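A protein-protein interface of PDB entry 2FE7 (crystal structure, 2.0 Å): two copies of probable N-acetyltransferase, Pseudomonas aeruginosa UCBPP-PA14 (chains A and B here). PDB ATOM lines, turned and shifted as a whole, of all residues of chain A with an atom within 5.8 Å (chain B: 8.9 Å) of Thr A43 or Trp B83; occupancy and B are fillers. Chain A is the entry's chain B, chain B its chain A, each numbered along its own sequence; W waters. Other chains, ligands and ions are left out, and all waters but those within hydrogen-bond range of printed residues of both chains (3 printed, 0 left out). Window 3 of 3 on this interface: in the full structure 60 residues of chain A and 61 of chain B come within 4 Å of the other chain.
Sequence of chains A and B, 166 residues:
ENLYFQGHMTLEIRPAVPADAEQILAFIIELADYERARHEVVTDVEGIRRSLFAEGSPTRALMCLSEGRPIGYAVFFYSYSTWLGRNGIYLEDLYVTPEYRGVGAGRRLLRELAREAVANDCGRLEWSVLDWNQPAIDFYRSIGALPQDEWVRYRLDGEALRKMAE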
ATOM      1  N   LEU A  25     -14.697 -24.491  -2.702  1.00  0.00           N
ATOM      2  CA  LEU A  25     -14.490 -23.209  -3.365  1.00  0.00           C
ATOM      3  C   LEU A  25     -14.116 -22.127  -2.361  1.00  0.00           C
ATOM      4  O   LEU A  25     -13.183 -21.360  -2.601  1.00  0.00           O
ATOM      5  CB  LEU A  25     -15.711 -22.783  -4.186  1.00  0.00           C
ATOM      6  CG  LEU A  25     -15.601 -21.422  -4.888  1.00  0.00           C
ATOM      7  CD1 LEU A  25     -14.409 -21.371  -5.868  1.00  0.00           C
ATOM      8  CD2 LEU A  25     -16.906 -21.057  -5.576  1.00  0.00           C
ATOM      9  N   ILE A  28     -10.571 -22.752  -1.504  1.00  0.00           N
ATOM     10  CA  ILE A  28      -9.738 -22.413  -2.665  1.00  0.00           C
ATOM     11  C   ILE A  28      -9.450 -20.912  -2.694  1.00  0.00           C
ATOM     12  O   ILE A  28      -8.317 -20.491  -2.930  1.00  0.00           O
ATOM     13  CB  ILE A  28     -10.396 -22.837  -4.004  1.00  0.00           C
ATOM     14  CG1 ILE A  28     -10.287 -24.357  -4.186  1.00  0.00           C
ATOM     15  CG2 ILE A  28      -9.723 -22.099  -5.193  1.00  0.00           C
ATOM     16  CD1 ILE A  28     -11.332 -24.954  -5.130  1.00  0.00           C
ATOM     17  N   LEU A  31      -7.042 -19.931   0.167  1.00  0.00           N
ATOM     18  CA  LEU A  31      -5.673 -20.327  -0.171  1.00  0.00           C
ATOM     19  C   LEU A  31      -5.073 -19.385  -1.215  1.00  0.00           C
ATOM     20  O   LEU A  31      -3.951 -18.904  -1.044  1.00  0.00           O
ATOM     21  CB  LEU A  31      -5.603 -21.788  -0.628  1.00  0.00           C
ATOM     22  CG  LEU A  31      -4.225 -22.326  -1.042  1.00  0.00           C
ATOM     23  CD1 LEU A  31      -3.180 -22.204   0.072  1.00  0.00           C
ATOM     24  CD2 LEU A  31      -4.342 -23.775  -1.510  1.00  0.00           C
ATOM     25  N   ALA A  32      -5.835 -19.106  -2.272  1.00  0.00           N
ATOM     26  CA  ALA A  32      -5.389 -18.205  -3.335  1.00  0.00           C
ATOM     27  C   ALA A  32      -5.083 -16.830  -2.765  1.00  0.00           C
ATOM     28  O   ALA A  32      -4.111 -16.195  -3.160  1.00  0.00           O
ATOM     29  CB  ALA A  32      -6.446 -18.097  -4.443  1.00  0.00           C
ATOM     30  N   GLU A  35      -1.906 -16.942  -1.090  1.00  0.00           N
ATOM     31  CA  GLU A  35      -0.885 -17.020  -2.128  1.00  0.00           C
ATOM     32  C   GLU A  35      -0.795 -15.748  -2.981  1.00  0.00           C
ATOM     33  O   GLU A  35      -0.116 -15.724  -4.012  1.00  0.00           O
ATOM     34  CB  GLU A  35      -1.107 -18.267  -2.973  1.00  0.00           C
ATOM     35  CG  GLU A  35      -0.761 -19.542  -2.200  1.00  0.00           C
ATOM     36  CD  GLU A  35      -1.122 -20.810  -2.948  1.00  0.00           C
ATOM     37  OE1 GLU A  35      -1.899 -20.755  -3.923  1.00  0.00           O
ATOM     38  OE2 GLU A  35      -0.625 -21.877  -2.555  1.00  0.00           O
ATOM     39  N   ALA A  37      -3.022 -14.252  -4.830  1.00  0.00           N
ATOM     40  CA  ALA A  37      -3.546 -14.544  -6.160  1.00  0.00           C
ATOM     41  C   ALA A  37      -5.062 -14.675  -6.156  1.00  0.00           C
ATOM     42  O   ALA A  37      -5.624 -15.379  -6.995  1.00  0.00           O
ATOM     43  CB  ALA A  37      -2.899 -15.813  -6.716  1.00  0.00           C
ATOM     44  N   GLU A  40      -7.032 -14.609  -9.294  1.00  0.00           N
ATOM     45  CA  GLU A  40      -6.868 -15.709 -10.239  1.00  0.00           C
ATOM     46  C   GLU A  40      -7.985 -16.763 -10.174  1.00  0.00           C
ATOM     47  O   GLU A  40      -8.124 -17.583 -11.092  1.00  0.00           O
ATOM     48  CB  GLU A  40      -5.487 -16.369 -10.091  1.00  0.00           C
ATOM     49  CG  GLU A  40      -4.290 -15.453 -10.392  1.00  0.00           C
ATOM     50  CD  GLU A  40      -4.180 -15.040 -11.864  1.00  0.00           C
ATOM     51  OE1 GLU A  40      -4.942 -15.544 -12.729  1.00  0.00           O
ATOM     52  OE2 GLU A  40      -3.321 -14.185 -12.163  1.00  0.00           O
ATOM     53  N   VAL A  41      -8.767 -16.744  -9.098  1.00  0.00           N
ATOM     54  CA  VAL A  41      -9.874 -17.697  -8.943  1.00  0.00           C
ATOM     55  C   VAL A  41     -11.039 -17.209  -9.786  1.00  0.00           C
ATOM     56  O   VAL A  41     -11.714 -16.246  -9.422  1.00  0.00           O
ATOM     57  CB  VAL A  41     -10.326 -17.864  -7.472  1.00  0.00           C
ATOM     58  CG1 VAL A  41     -11.430 -18.933  -7.376  1.00  0.00           C
ATOM     59  CG2 VAL A  41      -9.141 -18.244  -6.594  1.00  0.00           C
ATOM     60  N   VAL A  42     -11.270 -17.883 -10.907  1.00  0.00           N
ATOM     61  CA  VAL A  42     -12.273 -17.440 -11.867  1.00  0.00           C
ATOM     62  C   VAL A  42     -13.406 -18.456 -12.035  1.00  0.00           C
ATOM     63  O   VAL A  42     -14.361 -18.220 -12.770  1.00  0.00           O
ATOM     64  CB  VAL A  42     -11.633 -17.074 -13.247  1.00  0.00           C
ATOM     65  CG1 VAL A  42     -10.706 -15.874 -13.111  1.00  0.00           C
ATOM     66  CG2 VAL A  42     -10.894 -18.258 -13.842  1.00  0.00           C
ATOM     67  N   THR A  43     -13.297 -19.579 -11.337  1.00  0.00           N
ATOM     68  CA  THR A  43     -14.327 -20.617 -11.374  1.00  0.00           C
ATOM     69  C   THR A  43     -15.492 -20.259 -10.439  1.00  0.00           C
ATOM     70  O   THR A  43     -15.388 -19.321  -9.642  1.00  0.00           O
ATOM     71  CB  THR A  43     -13.737 -22.004 -10.993  1.00  0.00           C
ATOM     72  OG1 THR A  43     -14.735 -23.013 -11.151  1.00  0.00           O
ATOM     73  CG2 THR A  43     -13.237 -22.023  -9.546  1.00  0.00           C
ATOM     74  N   ASP A  44     -16.585 -21.011 -10.543  1.00  0.00           N
ATOM     75  CA  ASP A  44     -17.717 -20.886  -9.628  1.00  0.00           C
ATOM     76  C   ASP A  44     -18.045 -22.247  -9.008  1.00  0.00           C
ATOM     77  O   ASP A  44     -17.454 -23.264  -9.388  1.00  0.00           O
ATOM     78  CB  ASP A  44     -18.935 -20.269 -10.337  1.00  0.00           C
ATOM     79  CG  ASP A  44     -19.326 -21.005 -11.612  1.00  0.00           C
ATOM     80  OD1 ASP A  44     -18.996 -22.195 -11.771  1.00  0.00           O
ATOM     81  OD2 ASP A  44     -20.008 -20.387 -12.460  1.00  0.00           O
ATOM     82  N   VAL A  45     -18.970 -22.267  -8.051  1.00  0.00           N
ATOM     83  CA  VAL A  45     -19.283 -23.501  -7.319  1.00  0.00           C
ATOM     84  C   VAL A  45     -19.697 -24.670  -8.230  1.00  0.00           C
ATOM     85  O   VAL A  45     -19.257 -25.808  -8.030  1.00  0.00           O
ATOM     86  CB  VAL A  45     -20.313 -23.272  -6.177  1.00  0.00           C
ATOM     87  CG1 VAL A  45     -21.700 -22.900  -6.719  1.00  0.00           C
ATOM     88  CG2 VAL A  45     -20.382 -24.492  -5.269  1.00  0.00           C
ATOM     89  N   GLY A  47     -18.938 -25.002 -11.429  1.00  0.00           N
ATOM     90  CA  GLY A  47     -17.727 -25.387 -12.161  1.00  0.00           C
ATOM     91  C   GLY A  47     -16.894 -26.405 -11.388  1.00  0.00           C
ATOM     92  O   GLY A  47     -16.521 -27.449 -11.922  1.00  0.00           O
ATOM     93  N   ILE A  48     -16.609 -26.091 -10.128  1.00  0.00           N
ATOM     94  CA  ILE A  48     -15.933 -27.003  -9.194  1.00  0.00           C
ATOM     95  C   ILE A  48     -16.685 -28.332  -9.003  1.00  0.00           C
ATOM     96  O   ILE A  48     -16.107 -29.405  -9.192  1.00  0.00           O
ATOM     97  CB  ILE A  48     -15.707 -26.311  -7.812  1.00  0.00           C
ATOM     98  CG1 ILE A  48     -14.651 -25.191  -7.920  1.00  0.00           C
ATOM     99  CG2 ILE A  48     -15.389 -27.335  -6.694  1.00  0.00           C
ATOM    100  CD1 ILE A  48     -13.232 -25.653  -8.207  1.00  0.00           C
ATOM    101  N   ASP A  93      -3.395 -28.428  -4.162  1.00  0.00           N
ATOM    102  CA  ASP A  93      -3.770 -27.511  -3.083  1.00  0.00           C
ATOM    103  C   ASP A  93      -3.736 -28.255  -1.770  1.00  0.00           C
ATOM    104  O   ASP A  93      -4.223 -29.383  -1.668  1.00  0.00           O
ATOM    105  CB  ASP A  93      -5.202 -26.963  -3.250  1.00  0.00           C
ATOM    106  CG  ASP A  93      -5.338 -25.879  -4.329  1.00  0.00           C
ATOM    107  OD1 ASP A  93      -4.391 -25.606  -5.094  1.00  0.00           O
ATOM    108  OD2 ASP A  93      -6.444 -25.285  -4.408  1.00  0.00           O
ATOM    109  N   TYR B  80      -5.052 -30.564 -12.766  1.00  0.00           N
ATOM    110  CA  TYR B  80      -6.249 -29.823 -12.394  1.00  0.00           C
ATOM    111  C   TYR B  80      -5.864 -28.470 -11.807  1.00  0.00           C
ATOM    112  O   TYR B  80      -4.937 -28.367 -11.012  1.00  0.00           O
ATOM    113  CB  TYR B  80      -7.119 -30.627 -11.408  1.00  0.00           C
ATOM    114  CG  TYR B  80      -8.462 -29.992 -11.127  1.00  0.00           C
ATOM    115  CD1 TYR B  80      -9.517 -30.120 -12.038  1.00  0.00           C
ATOM    116  CD2 TYR B  80      -8.680 -29.244  -9.961  1.00  0.00           C
ATOM    117  CE1 TYR B  80     -10.758 -29.524 -11.800  1.00  0.00           C
ATOM    118  CE2 TYR B  80      -9.919 -28.638  -9.714  1.00  0.00           C
ATOM    119  CZ  TYR B  80     -10.954 -28.791 -10.636  1.00  0.00           C
ATOM    120  OH  TYR B  80     -12.180 -28.209 -10.410  1.00  0.00           O
ATOM    121  N   SER B  81      -6.583 -27.433 -12.231  1.00  0.00           N
ATOM    122  CA  SER B  81      -6.438 -26.106 -11.662  1.00  0.00           C
ATOM    123  C   SER B  81      -7.684 -25.774 -10.851  1.00  0.00           C
ATOM    124  O   SER B  81      -8.794 -25.674 -11.401  1.00  0.00           O
ATOM    125  CB  SER B  81      -6.266 -25.063 -12.763  1.00  0.00           C
ATOM    126  OG  SER B  81      -6.365 -23.764 -12.215  1.00  0.00           O
ATOM    127  N   THR B  82      -7.494 -25.604  -9.548  1.00  0.00           N
ATOM    128  CA  THR B  82      -8.586 -25.207  -8.659  1.00  0.00           C
ATOM    129  C   THR B  82      -9.002 -23.750  -8.908  1.00  0.00           C
ATOM    130  O   THR B  82     -10.145 -23.373  -8.655  1.00  0.00           O
ATOM    131  CB  THR B  82      -8.213 -25.393  -7.175  1.00  0.00           C
ATOM    132  OG1 THR B  82      -7.037 -24.629  -6.864  1.00  0.00           O
ATOM    133  CG2 THR B  82      -7.965 -26.859  -6.850  1.00  0.00           C
ATOM    134  N   TRP B  83      -8.079 -22.937  -9.414  1.00  0.00           N
ATOM    135  CA  TRP B  83      -8.391 -21.541  -9.707  1.00  0.00           C
ATOM    136  C   TRP B  83      -9.322 -21.406 -10.918  1.00  0.00           C
ATOM    137  O   TRP B  83     -10.211 -20.562 -10.930  1.00  0.00           O
ATOM    138  CB  TRP B  83      -7.111 -20.732  -9.917  1.00  0.00           C
ATOM    139  CG  TRP B  83      -6.239 -20.674  -8.699  1.00  0.00           C
ATOM    140  CD1 TRP B  83      -6.530 -21.160  -7.448  1.00  0.00           C
ATOM    141  CD2 TRP B  83      -4.940 -20.070  -8.599  1.00  0.00           C
ATOM    142  NE1 TRP B  83      -5.486 -20.913  -6.592  1.00  0.00           N
ATOM    143  CE2 TRP B  83      -4.501 -20.240  -7.264  1.00  0.00           C
ATOM    144  CE3 TRP B  83      -4.104 -19.401  -9.511  1.00  0.00           C
ATOM    145  CZ2 TRP B  83      -3.264 -19.762  -6.809  1.00  0.00           C
ATOM    146  CZ3 TRP B  83      -2.867 -18.927  -9.058  1.00  0.00           C
ATOM    147  CH2 TRP B  83      -2.459 -19.114  -7.717  1.00  0.00           C
ATOM    148  N   LEU B  84      -9.109 -22.264 -11.911  1.00  0.00           N
ATOM    149  CA  LEU B  84      -9.858 -22.258 -13.163  1.00  0.00           C
ATOM    150  C   LEU B  84     -11.068 -23.173 -13.091  1.00  0.00           C
ATOM    151  O   LEU B  84     -11.991 -23.054 -13.895  1.00  0.00           O
ATOM    152  CB  LEU B  84      -8.953 -22.738 -14.311  1.00  0.00           C
ATOM    153  CG  LEU B  84      -7.714 -21.923 -14.691  1.00  0.00           C
ATOM    154  CD1 LEU B  84      -7.111 -22.504 -15.961  1.00  0.00           C
ATOM    155  CD2 LEU B  84      -8.055 -20.436 -14.898  1.00  0.00           C
ATOM    156  N   GLY B  85     -11.043 -24.103 -12.134  1.00  0.00           N
ATOM    157  CA  GLY B  85     -12.057 -25.151 -12.043  1.00  0.00           C
ATOM    158  C   GLY B  85     -12.041 -26.003 -13.295  1.00  0.00           C
ATOM    159  O   GLY B  85     -13.090 -26.409 -13.790  1.00  0.00           O
ATOM    160  N   ARG B  86     -10.841 -26.279 -13.805  1.00  0.00           N
ATOM    161  CA  ARG B  86     -10.685 -26.995 -15.066  1.00  0.00           C
ATOM    162  C   ARG B  86      -9.523 -27.973 -15.018  1.00  0.00           C
ATOM    163  O   ARG B  86      -8.500 -27.708 -14.380  1.00  0.00           O
ATOM    164  CB  ARG B  86     -10.444 -26.010 -16.214  1.00  0.00           C
ATOM    165  CG  ARG B  86     -11.639 -25.163 -16.608  1.00  0.00           C
ATOM    166  CD  ARG B  86     -11.250 -24.146 -17.672  1.00  0.00           C
ATOM    167  NE  ARG B  86     -11.313 -24.724 -19.010  1.00  0.00           N
ATOM    168  CZ  ARG B  86     -11.002 -24.081 -20.135  1.00  0.00           C
ATOM    169  NH1 ARG B  86     -10.593 -22.815 -20.106  1.00  0.00           N
ATOM    170  NH2 ARG B  86     -11.113 -24.708 -21.303  1.00  0.00           N
ATOM    171  N   ARG B 124      -4.982 -25.325 -19.261  1.00  0.00           N
ATOM    172  CA  ARG B 124      -3.524 -25.193 -19.309  1.00  0.00           C
ATOM    173  C   ARG B 124      -2.876 -26.433 -19.905  1.00  0.00           C
ATOM    174  O   ARG B 124      -3.356 -27.553 -19.705  1.00  0.00           O
ATOM    175  CB  ARG B 124      -2.949 -24.859 -17.909  1.00  0.00           C
ATOM    176  CG  ARG B 124      -3.811 -23.791 -17.207  1.00  0.00           C
ATOM    177  CD  ARG B 124      -3.204 -22.931 -16.108  1.00  0.00           C
ATOM    178  NE  ARG B 124      -3.002 -23.647 -14.877  1.00  0.00           N
ATOM    179  CZ  ARG B 124      -3.210 -23.173 -13.650  1.00  0.00           C
ATOM    180  NH1 ARG B 124      -3.691 -21.953 -13.419  1.00  0.00           N
ATOM    181  NH2 ARG B 124      -2.943 -23.963 -12.634  1.00  0.00           N
ATOM    182  N   GLN B 148       6.658 -20.259 -15.215  1.00  0.00           N
ATOM    183  CA  GLN B 148       5.966 -20.123 -13.940  1.00  0.00           C
ATOM    184  C   GLN B 148       7.030 -20.172 -12.867  1.00  0.00           C
ATOM    185  O   GLN B 148       7.104 -21.123 -12.070  1.00  0.00           O
ATOM    186  CB  GLN B 148       4.946 -21.262 -13.772  1.00  0.00           C
ATOM    187  CG  GLN B 148       3.991 -21.407 -14.938  1.00  0.00           C
ATOM    188  CD  GLN B 148       3.295 -20.101 -15.289  1.00  0.00           C
ATOM    189  OE1 GLN B 148       3.463 -19.564 -16.391  1.00  0.00           O
ATOM    190  NE2 GLN B 148       2.517 -19.577 -14.350  1.00  0.00           N
ATOM    191  N   GLU B 150       7.861 -18.426 -10.152  1.00  0.00           N
ATOM    192  CA  GLU B 150       7.696 -18.116  -8.732  1.00  0.00           C
ATOM    193  C   GLU B 150       7.574 -19.381  -7.871  1.00  0.00           C
ATOM    194  O   GLU B 150       7.726 -19.323  -6.657  1.00  0.00           O
ATOM    195  CB  GLU B 150       6.485 -17.216  -8.513  1.00  0.00           C
ATOM    196  CG  GLU B 150       6.694 -15.794  -9.010  1.00  0.00           C
ATOM    197  CD  GLU B 150       5.815 -14.803  -8.274  1.00  0.00           C
ATOM    198  OE1 GLU B 150       6.373 -13.836  -7.716  1.00  0.00           O
ATOM    199  OE2 GLU B 150       4.578 -15.003  -8.243  1.00  0.00           O
ATOM    200  N   TRP B 151       7.314 -20.517  -8.512  1.00  0.00           N
ATOM    201  CA  TRP B 151       7.073 -21.779  -7.811  1.00  0.00           C
ATOM    202  C   TRP B 151       8.317 -22.647  -7.787  1.00  0.00           C
ATOM    203  O   TRP B 151       9.091 -22.656  -8.745  1.00  0.00           O
ATOM    204  CB  TRP B 151       5.942 -22.556  -8.490  1.00  0.00           C
ATOM    205  CG  TRP B 151       4.598 -21.862  -8.441  1.00  0.00           C
ATOM    206  CD1 TRP B 151       4.077 -21.009  -9.380  1.00  0.00           C
ATOM    207  CD2 TRP B 151       3.614 -21.963  -7.401  1.00  0.00           C
ATOM    208  NE1 TRP B 151       2.828 -20.571  -8.985  1.00  0.00           N
ATOM    209  CE2 TRP B 151       2.516 -21.147  -7.780  1.00  0.00           C
ATOM    210  CE3 TRP B 151       3.545 -22.671  -6.193  1.00  0.00           C
ATOM    211  CZ2 TRP B 151       1.370 -21.010  -6.986  1.00  0.00           C
ATOM    212  CZ3 TRP B 151       2.396 -22.535  -5.396  1.00  0.00           C
ATOM    213  CH2 TRP B 151       1.329 -21.708  -5.800  1.00  0.00           C
HETATM  214  O   HOH W   1      -3.296 -22.652  -4.711  1.00  0.00           O
HETATM  215  O   HOH W   2     -15.044 -23.625 -13.806  1.00  0.00           O
HETATM  216  O   HOH W   3      -6.248 -22.288  -4.250  1.00  0.00           O
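O of Trp B83 sits at hydrogen-bond distance from N of Thr A43, 3.3 Å away. N of Val A42 sits at hydrogen-bond distance from O of Trp B83 (2.9 Å). The side-chain carboxylate (OD2) of Asp A93 is in hydrogen-bond range of the side-chain hydroxyl (OG1) of Thr B82.
OG of Ser B81 is in hydrogen-bond range of N of Leu B84 (3.1 Å). The backbone carbonyl oxygen (O) of Ala A32 sits at hydrogen-bond distance from the backbone NH (N) of Ala A37 (2.8 Å). The side-chain hydroxyl of Ser B81 sits close to the backbone NH of Trp B83 (3.4 Å).
Among the printed residues, merely in contact across the chains: Ile A28 with Thr B82 (3.7 Å), Ala A32 with Trp B83 (3.7 Å), Glu A35 with Trp B83 (3.3 Å), Glu A35 with Trp B151 (3.8 Å), Ala A37 with Trp B83 (3.5 Å), Glu A40 with Trp B83 (3.4 Å), Val A41 with Trp B83 (3.5 Å), Val A42 with Leu B84 (3.7 Å), Thr A43 with Thr B82 (3.5 Å), Thr A43 with Leu B84 (3.5 Å), Thr A43 with Gly B85 (3.5 Å), Ile A48 with Tyr B80 (3.5 Å) and Ile A48 with Thr B82 (3.9 Å).
Of chain B, only Thr B82, Trp B83, Leu B84 and Gly B85 come within 4 Å of Thr A43. No residue of chain B comes within 4 Å of Gly A47. Of the printed residues of chain B, Ala A37 touches Trp B83 (3.5 Å). Printed residues of chain A within 4 Å of Trp B151: Glu A35. Printed residues of chain A within 4 Å of Leu B84: Val A42 and Thr A43. Glu B150 touches none of the printed residues of chain A. The nearest residue of chain B that does not touch Thr A43 is Arg B86 (5.7 Å). The nearest residue of chain A that does not touch Trp B83 is Ile A28 (4.02 Å).
Of the 15 printed residues of chain A, 10 touch a printed residue of chain B. Printed residues of chain A that touch a printed residue of chain B: Ile A28, Ala A32, Glu A35, Ala A37, Glu A40, Val A41, Val A42, Thr A43, Ile A48 and Asp A93. Among the printed residues, 16 pairs touch across the chains.
No position is printed for both chains.
Water W1 lies within hydrogen-bond range of the side-chain carboxylate of Glu A35 (2.5 Å), the side-chain carboxylate of Asp A93 (3.2 Å) and the indole nitrogen of Trp B83 (3.4 Å). Water W2 lies within hydrogen-bond range of OG1 of Thr A43, O of Leu B84 and O of Gly B85. Water W3 lies within hydrogen-bond range of NE1 of Trp B83 (2.8 Å), OD2 of Asp A93 (3.0 Å) and O of Ile A28 (3.0 Å).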
